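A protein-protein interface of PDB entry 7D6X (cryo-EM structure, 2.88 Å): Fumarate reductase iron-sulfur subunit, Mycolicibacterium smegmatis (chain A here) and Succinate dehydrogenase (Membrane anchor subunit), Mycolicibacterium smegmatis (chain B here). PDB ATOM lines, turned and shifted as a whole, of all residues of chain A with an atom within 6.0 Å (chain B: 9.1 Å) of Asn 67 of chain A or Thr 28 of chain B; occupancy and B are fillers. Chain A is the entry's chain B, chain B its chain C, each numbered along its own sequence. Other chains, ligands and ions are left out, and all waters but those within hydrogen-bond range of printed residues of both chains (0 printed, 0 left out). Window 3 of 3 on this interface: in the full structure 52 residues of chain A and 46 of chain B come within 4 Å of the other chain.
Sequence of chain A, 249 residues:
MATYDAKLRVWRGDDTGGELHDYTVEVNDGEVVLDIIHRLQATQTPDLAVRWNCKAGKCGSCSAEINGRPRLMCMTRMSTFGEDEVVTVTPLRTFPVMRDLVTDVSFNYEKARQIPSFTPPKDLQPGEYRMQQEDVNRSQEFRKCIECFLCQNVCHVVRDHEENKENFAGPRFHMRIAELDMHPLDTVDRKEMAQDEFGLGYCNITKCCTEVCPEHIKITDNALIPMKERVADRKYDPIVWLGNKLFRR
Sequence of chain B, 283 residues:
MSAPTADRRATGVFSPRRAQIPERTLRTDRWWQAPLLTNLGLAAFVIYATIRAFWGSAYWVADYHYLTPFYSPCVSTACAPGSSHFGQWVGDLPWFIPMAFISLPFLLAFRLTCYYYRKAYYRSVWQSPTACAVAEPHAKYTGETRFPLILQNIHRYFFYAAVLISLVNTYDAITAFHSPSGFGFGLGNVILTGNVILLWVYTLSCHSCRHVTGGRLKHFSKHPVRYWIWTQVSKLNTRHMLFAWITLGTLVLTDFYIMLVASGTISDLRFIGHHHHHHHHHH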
ATOM      1  N   GLU A  65      26.529 -21.667 -37.860  1.00  0.00           N
ATOM      2  CA  GLU A  65      26.037 -21.328 -36.526  1.00  0.00           C
ATOM      3  C   GLU A  65      27.250 -21.105 -35.633  1.00  0.00           C
ATOM      4  O   GLU A  65      27.864 -22.065 -35.162  1.00  0.00           O
ATOM      5  CB  GLU A  65      25.131 -22.418 -35.988  1.00  0.00           C
ATOM      6  CG  GLU A  65      23.873 -22.588 -36.801  1.00  0.00           C
ATOM      7  CD  GLU A  65      22.783 -23.273 -36.030  1.00  0.00           C
ATOM      8  OE1 GLU A  65      23.082 -23.830 -34.958  1.00  0.00           O
ATOM      9  OE2 GLU A  65      21.627 -23.250 -36.491  1.00  0.00           O
ATOM     10  N   ILE A  66      27.576 -19.838 -35.383  1.00  0.00           N
ATOM     11  CA  ILE A  66      28.912 -19.497 -34.907  1.00  0.00           C
ATOM     12  C   ILE A  66      29.057 -19.796 -33.424  1.00  0.00           C
ATOM     13  O   ILE A  66      30.102 -20.282 -32.981  1.00  0.00           O
ATOM     14  CB  ILE A  66      29.240 -18.032 -35.218  1.00  0.00           C
ATOM     15  CG1 ILE A  66      29.148 -17.785 -36.719  1.00  0.00           C
ATOM     16  CG2 ILE A  66      30.628 -17.701 -34.728  1.00  0.00           C
ATOM     17  CD1 ILE A  66      29.972 -18.729 -37.524  1.00  0.00           C
ATOM     18  N   ASN A  67      28.058 -19.453 -32.622  1.00  0.00           N
ATOM     19  CA  ASN A  67      28.082 -19.840 -31.216  1.00  0.00           C
ATOM     20  C   ASN A  67      26.682 -20.183 -30.745  1.00  0.00           C
ATOM     21  O   ASN A  67      26.249 -19.767 -29.668  1.00  0.00           O
ATOM     22  CB  ASN A  67      28.705 -18.747 -30.354  1.00  0.00           C
ATOM     23  CG  ASN A  67      29.580 -19.304 -29.262  1.00  0.00           C
ATOM     24  OD1 ASN A  67      29.624 -20.508 -29.044  1.00  0.00           O
ATOM     25  ND2 ASN A  67      30.298 -18.431 -28.580  1.00  0.00           N
ATOM     26  N   GLY A  68      25.957 -20.944 -31.551  1.00  0.00           N
ATOM     27  CA  GLY A  68      24.544 -21.146 -31.354  1.00  0.00           C
ATOM     28  C   GLY A  68      23.670 -20.176 -32.109  1.00  0.00           C
ATOM     29  O   GLY A  68      22.447 -20.341 -32.105  1.00  0.00           O
ATOM     30  N   ARG A  69      24.258 -19.181 -32.765  1.00  0.00           N
ATOM     31  CA  ARG A  69      23.518 -18.163 -33.489  1.00  0.00           C
ATOM     32  C   ARG A  69      23.795 -18.309 -34.975  1.00  0.00           C
ATOM     33  O   ARG A  69      24.966 -18.389 -35.365  1.00  0.00           O
ATOM     34  CB  ARG A  69      23.918 -16.767 -33.014  1.00  0.00           C
ATOM     35  CG  ARG A  69      23.691 -16.499 -31.538  1.00  0.00           C
ATOM     36  CD  ARG A  69      22.220 -16.545 -31.188  1.00  0.00           C
ATOM     37  NE  ARG A  69      21.435 -15.576 -31.944  1.00  0.00           N
ATOM     38  CZ  ARG A  69      21.252 -14.316 -31.571  1.00  0.00           C
ATOM     39  NH1 ARG A  69      21.804 -13.871 -30.452  1.00  0.00           N
ATOM     40  NH2 ARG A  69      20.520 -13.504 -32.322  1.00  0.00           N
ATOM     41  N   PHE A  81      33.951 -12.222 -29.131  1.00  0.00           N
ATOM     42  CA  PHE A  81      34.206 -13.266 -28.157  1.00  0.00           C
ATOM     43  C   PHE A  81      35.434 -12.921 -27.332  1.00  0.00           C
ATOM     44  O   PHE A  81      36.420 -12.399 -27.857  1.00  0.00           O
ATOM     45  CB  PHE A  81      34.407 -14.605 -28.863  1.00  0.00           C
ATOM     46  CG  PHE A  81      33.407 -14.868 -29.944  1.00  0.00           C
ATOM     47  CD1 PHE A  81      32.114 -15.230 -29.631  1.00  0.00           C
ATOM     48  CD2 PHE A  81      33.757 -14.745 -31.271  1.00  0.00           C
ATOM     49  CE1 PHE A  81      31.193 -15.467 -30.621  1.00  0.00           C
ATOM     50  CE2 PHE A  81      32.841 -14.980 -32.261  1.00  0.00           C
ATOM     51  CZ  PHE A  81      31.558 -15.343 -31.937  1.00  0.00           C
ATOM     52  N   GLU A  85      37.444 -17.553 -24.075  1.00  0.00           N
ATOM     53  CA  GLU A  85      36.246 -18.353 -24.253  1.00  0.00           C
ATOM     54  C   GLU A  85      36.323 -19.151 -25.547  1.00  0.00           C
ATOM     55  O   GLU A  85      37.022 -18.776 -26.492  1.00  0.00           O
ATOM     56  CB  GLU A  85      34.996 -17.476 -24.252  1.00  0.00           C
ATOM     57  CG  GLU A  85      34.650 -16.863 -25.584  1.00  0.00           C
ATOM     58  CD  GLU A  85      33.316 -16.148 -25.555  1.00  0.00           C
ATOM     59  OE1 GLU A  85      33.112 -15.307 -24.656  1.00  0.00           O
ATOM     60  OE2 GLU A  85      32.469 -16.429 -26.425  1.00  0.00           O
ATOM     61  N   VAL A  86      35.596 -20.261 -25.574  1.00  0.00           N
ATOM     62  CA  VAL A  86      35.625 -21.210 -26.679  1.00  0.00           C
ATOM     63  C   VAL A  86      34.584 -20.808 -27.707  1.00  0.00           C
ATOM     64  O   VAL A  86      33.482 -20.373 -27.359  1.00  0.00           O
ATOM     65  CB  VAL A  86      35.381 -22.637 -26.160  1.00  0.00           C
ATOM     66  CG1 VAL A  86      35.456 -23.639 -27.284  1.00  0.00           C
ATOM     67  CG2 VAL A  86      36.389 -22.969 -25.089  1.00  0.00           C
ATOM     68  N   VAL A  87      34.933 -20.945 -28.982  1.00  0.00           N
ATOM     69  CA  VAL A  87      34.033 -20.624 -30.083  1.00  0.00           C
ATOM     70  C   VAL A  87      33.622 -21.929 -30.746  1.00  0.00           C
ATOM     71  O   VAL A  87      34.478 -22.702 -31.183  1.00  0.00           O
ATOM     72  CB  VAL A  87      34.690 -19.676 -31.095  1.00  0.00           C
ATOM     73  CG1 VAL A  87      33.730 -19.363 -32.220  1.00  0.00           C
ATOM     74  CG2 VAL A  87      35.146 -18.418 -30.409  1.00  0.00           C
ATOM     75  N   THR A  88      32.318 -22.165 -30.840  1.00  0.00           N
ATOM     76  CA  THR A  88      31.766 -23.445 -31.278  1.00  0.00           C
ATOM     77  C   THR A  88      31.071 -23.275 -32.622  1.00  0.00           C
ATOM     78  O   THR A  88      29.938 -22.798 -32.684  1.00  0.00           O
ATOM     79  CB  THR A  88      30.798 -23.989 -30.239  1.00  0.00           C
ATOM     80  OG1 THR A  88      31.507 -24.263 -29.028  1.00  0.00           O
ATOM     81  CG2 THR A  88      30.151 -25.262 -30.738  1.00  0.00           C
ATOM     82  N   VAL A  89      31.727 -23.719 -33.690  1.00  0.00           N
ATOM     83  CA  VAL A  89      31.211 -23.585 -35.048  1.00  0.00           C
ATOM     84  C   VAL A  89      30.616 -24.916 -35.488  1.00  0.00           C
ATOM     85  O   VAL A  89      31.287 -25.953 -35.434  1.00  0.00           O
ATOM     86  CB  VAL A  89      32.309 -23.132 -36.019  1.00  0.00           C
ATOM     87  CG1 VAL A  89      31.741 -22.966 -37.403  1.00  0.00           C
ATOM     88  CG2 VAL A  89      32.931 -21.846 -35.542  1.00  0.00           C
ATOM     89  N   THR B  25      20.360 -26.455 -27.351  1.00  0.00           N
ATOM     90  CA  THR B  25      20.926 -25.272 -27.978  1.00  0.00           C
ATOM     91  C   THR B  25      22.400 -25.204 -27.622  1.00  0.00           C
ATOM     92  O   THR B  25      22.824 -25.717 -26.584  1.00  0.00           O
ATOM     93  CB  THR B  25      20.226 -23.987 -27.536  1.00  0.00           C
ATOM     94  OG1 THR B  25      20.815 -22.873 -28.212  1.00  0.00           O
ATOM     95  CG2 THR B  25      20.365 -23.789 -26.038  1.00  0.00           C
ATOM     96  N   LEU B  26      23.174 -24.578 -28.499  1.00  0.00           N
ATOM     97  CA  LEU B  26      24.582 -24.329 -28.240  1.00  0.00           C
ATOM     98  C   LEU B  26      24.844 -22.898 -27.803  1.00  0.00           C
ATOM     99  O   LEU B  26      26.006 -22.516 -27.651  1.00  0.00           O
ATOM    100  CB  LEU B  26      25.411 -24.656 -29.481  1.00  0.00           C
ATOM    101  CG  LEU B  26      25.756 -26.126 -29.701  1.00  0.00           C
ATOM    102  CD1 LEU B  26      26.413 -26.305 -31.041  1.00  0.00           C
ATOM    103  CD2 LEU B  26      26.663 -26.632 -28.610  1.00  0.00           C
ATOM    104  N   ARG B  27      23.795 -22.106 -27.599  1.00  0.00           N
ATOM    105  CA  ARG B  27      23.953 -20.732 -27.150  1.00  0.00           C
ATOM    106  C   ARG B  27      24.489 -20.696 -25.729  1.00  0.00           C
ATOM    107  O   ARG B  27      24.081 -21.481 -24.870  1.00  0.00           O
ATOM    108  CB  ARG B  27      22.624 -19.989 -27.223  1.00  0.00           C
ATOM    109  CG  ARG B  27      22.145 -19.728 -28.626  1.00  0.00           C
ATOM    110  CD  ARG B  27      20.854 -18.952 -28.635  1.00  0.00           C
ATOM    111  NE  ARG B  27      21.000 -17.653 -27.995  1.00  0.00           N
ATOM    112  CZ  ARG B  27      20.050 -16.728 -27.967  1.00  0.00           C
ATOM    113  NH1 ARG B  27      18.884 -16.955 -28.545  1.00  0.00           N
ATOM    114  NH2 ARG B  27      20.267 -15.573 -27.360  1.00  0.00           N
ATOM    115  N   THR B  28      25.414 -19.772 -25.487  1.00  0.00           N
ATOM    116  CA  THR B  28      26.067 -19.627 -24.197  1.00  0.00           C
ATOM    117  C   THR B  28      25.649 -18.357 -23.473  1.00  0.00           C
ATOM    118  O   THR B  28      26.193 -18.055 -22.408  1.00  0.00           O
ATOM    119  CB  THR B  28      27.585 -19.650 -24.376  1.00  0.00           C
ATOM    120  OG1 THR B  28      27.941 -18.870 -25.522  1.00  0.00           O
ATOM    121  CG2 THR B  28      28.071 -21.066 -24.573  1.00  0.00           C
ATOM    122  N   ASP B  29      24.696 -17.612 -24.017  1.00  0.00           N
ATOM    123  CA  ASP B  29      24.277 -16.356 -23.421  1.00  0.00           C
ATOM    124  C   ASP B  29      23.082 -16.589 -22.502  1.00  0.00           C
ATOM    125  O   ASP B  29      22.701 -17.724 -22.205  1.00  0.00           O
ATOM    126  CB  ASP B  29      23.971 -15.332 -24.509  1.00  0.00           C
ATOM    127  CG  ASP B  29      22.876 -15.782 -25.438  1.00  0.00           C
ATOM    128  OD1 ASP B  29      22.085 -14.931 -25.888  1.00  0.00           O
ATOM    129  OD2 ASP B  29      22.803 -16.991 -25.720  1.00  0.00           O
ATOM    130  N   ARG B  30      22.488 -15.503 -22.029  1.00  0.00           N
ATOM    131  CA  ARG B  30      21.386 -15.560 -21.072  1.00  0.00           C
ATOM    132  C   ARG B  30      20.053 -15.415 -21.803  1.00  0.00           C
ATOM    133  O   ARG B  30      19.276 -14.494 -21.573  1.00  0.00           O
ATOM    134  CB  ARG B  30      21.568 -14.477 -20.017  1.00  0.00           C
ATOM    135  CG  ARG B  30      21.264 -14.904 -18.609  1.00  0.00           C
ATOM    136  CD  ARG B  30      21.811 -13.903 -17.607  1.00  0.00           C
ATOM    137  NE  ARG B  30      21.410 -12.538 -17.934  1.00  0.00           N
ATOM    138  CZ  ARG B  30      22.258 -11.542 -18.163  1.00  0.00           C
ATOM    139  NH1 ARG B  30      23.565 -11.748 -18.087  1.00  0.00           N
ATOM    140  NH2 ARG B  30      21.801 -10.335 -18.461  1.00  0.00           N
ATOM    141  N   TRP B  31      19.801 -16.367 -22.702  1.00  0.00           N
ATOM    142  CA  TRP B  31      18.681 -16.282 -23.632  1.00  0.00           C
ATOM    143  C   TRP B  31      17.327 -16.412 -22.953  1.00  0.00           C
ATOM    144  O   TRP B  31      16.311 -16.099 -23.581  1.00  0.00           O
ATOM    145  CB  TRP B  31      18.815 -17.360 -24.707  1.00  0.00           C
ATOM    146  CG  TRP B  31      19.089 -18.715 -24.149  1.00  0.00           C
ATOM    147  CD1 TRP B  31      20.306 -19.282 -23.944  1.00  0.00           C
ATOM    148  CD2 TRP B  31      18.121 -19.673 -23.712  1.00  0.00           C
ATOM    149  NE1 TRP B  31      20.160 -20.534 -23.408  1.00  0.00           N
ATOM    150  CE2 TRP B  31      18.825 -20.795 -23.254  1.00  0.00           C
ATOM    151  CE3 TRP B  31      16.728 -19.687 -23.664  1.00  0.00           C
ATOM    152  CZ2 TRP B  31      18.185 -21.920 -22.758  1.00  0.00           C
ATOM    153  CZ3 TRP B  31      16.095 -20.803 -23.169  1.00  0.00           C
ATOM    154  CH2 TRP B  31      16.823 -21.904 -22.723  1.00  0.00           C
ATOM    155  N   TRP B  32      17.283 -16.863 -21.707  1.00  0.00           N
ATOM    156  CA  TRP B  32      16.033 -17.037 -20.988  1.00  0.00           C
ATOM    157  C   TRP B  32      15.621 -15.801 -20.209  1.00  0.00           C
ATOM    158  O   TRP B  32      14.714 -15.885 -19.378  1.00  0.00           O
ATOM    159  CB  TRP B  32      16.143 -18.224 -20.034  1.00  0.00           C
ATOM    160  CG  TRP B  32      17.456 -18.299 -19.345  1.00  0.00           C
ATOM    161  CD1 TRP B  32      18.513 -19.085 -19.685  1.00  0.00           C
ATOM    162  CD2 TRP B  32      17.862 -17.558 -18.191  1.00  0.00           C
ATOM    163  NE1 TRP B  32      19.553 -18.882 -18.815  1.00  0.00           N
ATOM    164  CE2 TRP B  32      19.177 -17.946 -17.889  1.00  0.00           C
ATOM    165  CE3 TRP B  32      17.240 -16.601 -17.388  1.00  0.00           C
ATOM    166  CZ2 TRP B  32      19.879 -17.417 -16.814  1.00  0.00           C
ATOM    167  CZ3 TRP B  32      17.939 -16.072 -16.327  1.00  0.00           C
ATOM    168  CH2 TRP B  32      19.243 -16.481 -16.049  1.00  0.00           C
ATOM    169  N   ALA B 133      17.103 -19.688 -31.487  1.00  0.00           N
ATOM    170  CA  ALA B 133      17.538 -20.978 -32.006  1.00  0.00           C
ATOM    171  C   ALA B 133      17.662 -21.992 -30.884  1.00  0.00           C
ATOM    172  O   ALA B 133      18.663 -22.697 -30.759  1.00  0.00           O
ATOM    173  CB  ALA B 133      18.851 -20.842 -32.763  1.00  0.00           C
ATOM    174  N   VAL B 134      16.638 -22.078 -30.043  1.00  0.00           N
ATOM    175  CA  VAL B 134      16.585 -23.045 -28.955  1.00  0.00           C
ATOM    176  C   VAL B 134      15.479 -24.042 -29.261  1.00  0.00           C
ATOM    177  O   VAL B 134      14.386 -23.653 -29.687  1.00  0.00           O
ATOM    178  CB  VAL B 134      16.359 -22.359 -27.599  1.00  0.00           C
ATOM    179  CG1 VAL B 134      16.321 -23.387 -26.494  1.00  0.00           C
ATOM    180  CG2 VAL B 134      17.459 -21.360 -27.344  1.00  0.00           C
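O of Leu 26 of chain B lies close to O of Asn 67 of chain A, 3.4 Å away.
Asn 67 of chain A touches three residues of chain B. Gly 68 of chain A touches just these residues of chain B: Leu 26, Arg 27 and Ala 133. Of the printed residues of chain B, Arg 69 of chain A touches Arg 27 (3.6 Å). Phe 81 of chain A touches none of the printed residues of chain B. Of the printed residues of chain B, Thr 88 of chain A touches Leu 26. Of the printed residues of chain A, Leu 26 of chain B touches Asn 67 (3.4 Å), Gly 68 (3.97 Å) and Thr 88 (3.9 Å). Of the printed residues of chain A, Arg 27 of chain B touches Asn 67 (3.5 Å), Gly 68 (3.5 Å) and Arg 69 (3.6 Å). Thr 28 of chain B touches just one residue of chain A: Asn 67 (3.9 Å). Of the printed residues of chain A, Ala 133 of chain B touches Gly 68. The nearest residue of chain A that does not touch Thr 28 of chain B is Glu 85 of chain A (5.2 Å).
The backbone carbonyl oxygen (O) of Ile 66 of chain A lies close to the backbone carbonyl oxygen (O) of Thr 88 of chain A (2.5 Å). The side-chain hydroxyl (OG1) of Thr 25 of chain B lies within hydrogen-bond range of the backbone NH (N) of Arg 27 of chain B (3.1 Å). O of Ala 133 of chain B is in hydrogen-bond range of OG1 of Thr 25 of chain B. The guanidinium group of Arg 27 of chain B is in salt-bridge range of the side-chain carboxylate of Asp 29 of chain B (2.4 Å).
Among the printed residues, pairs that only touch across the chains: Asn 67 of chain A with Arg 27 of chain B, Gly 68 of chain A with Arg 27 of chain B, Arg 69 of chain A with Arg 27 of chain B, Gly 68 of chain A with Ala 133 of chain B, Asn 67 of chain A with Thr 28 of chain B, Thr 88 of chain A with Leu 26 of chain B and Gly 68 of chain A with Leu 26 of chain B.
Of the 11 printed residues of chain A, 4 touch a printed residue of chain B. Hydrophobic or aromatic side chains of chain B that line the printed part of chain A: Leu 26 and Ala 133. Among the printed residues, 8 pairs touch across the chains. Among the printed residues, no Asp or Glu carboxylate lies within 4 Å of a Lys or Arg side-chain nitrogen of the other chain.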
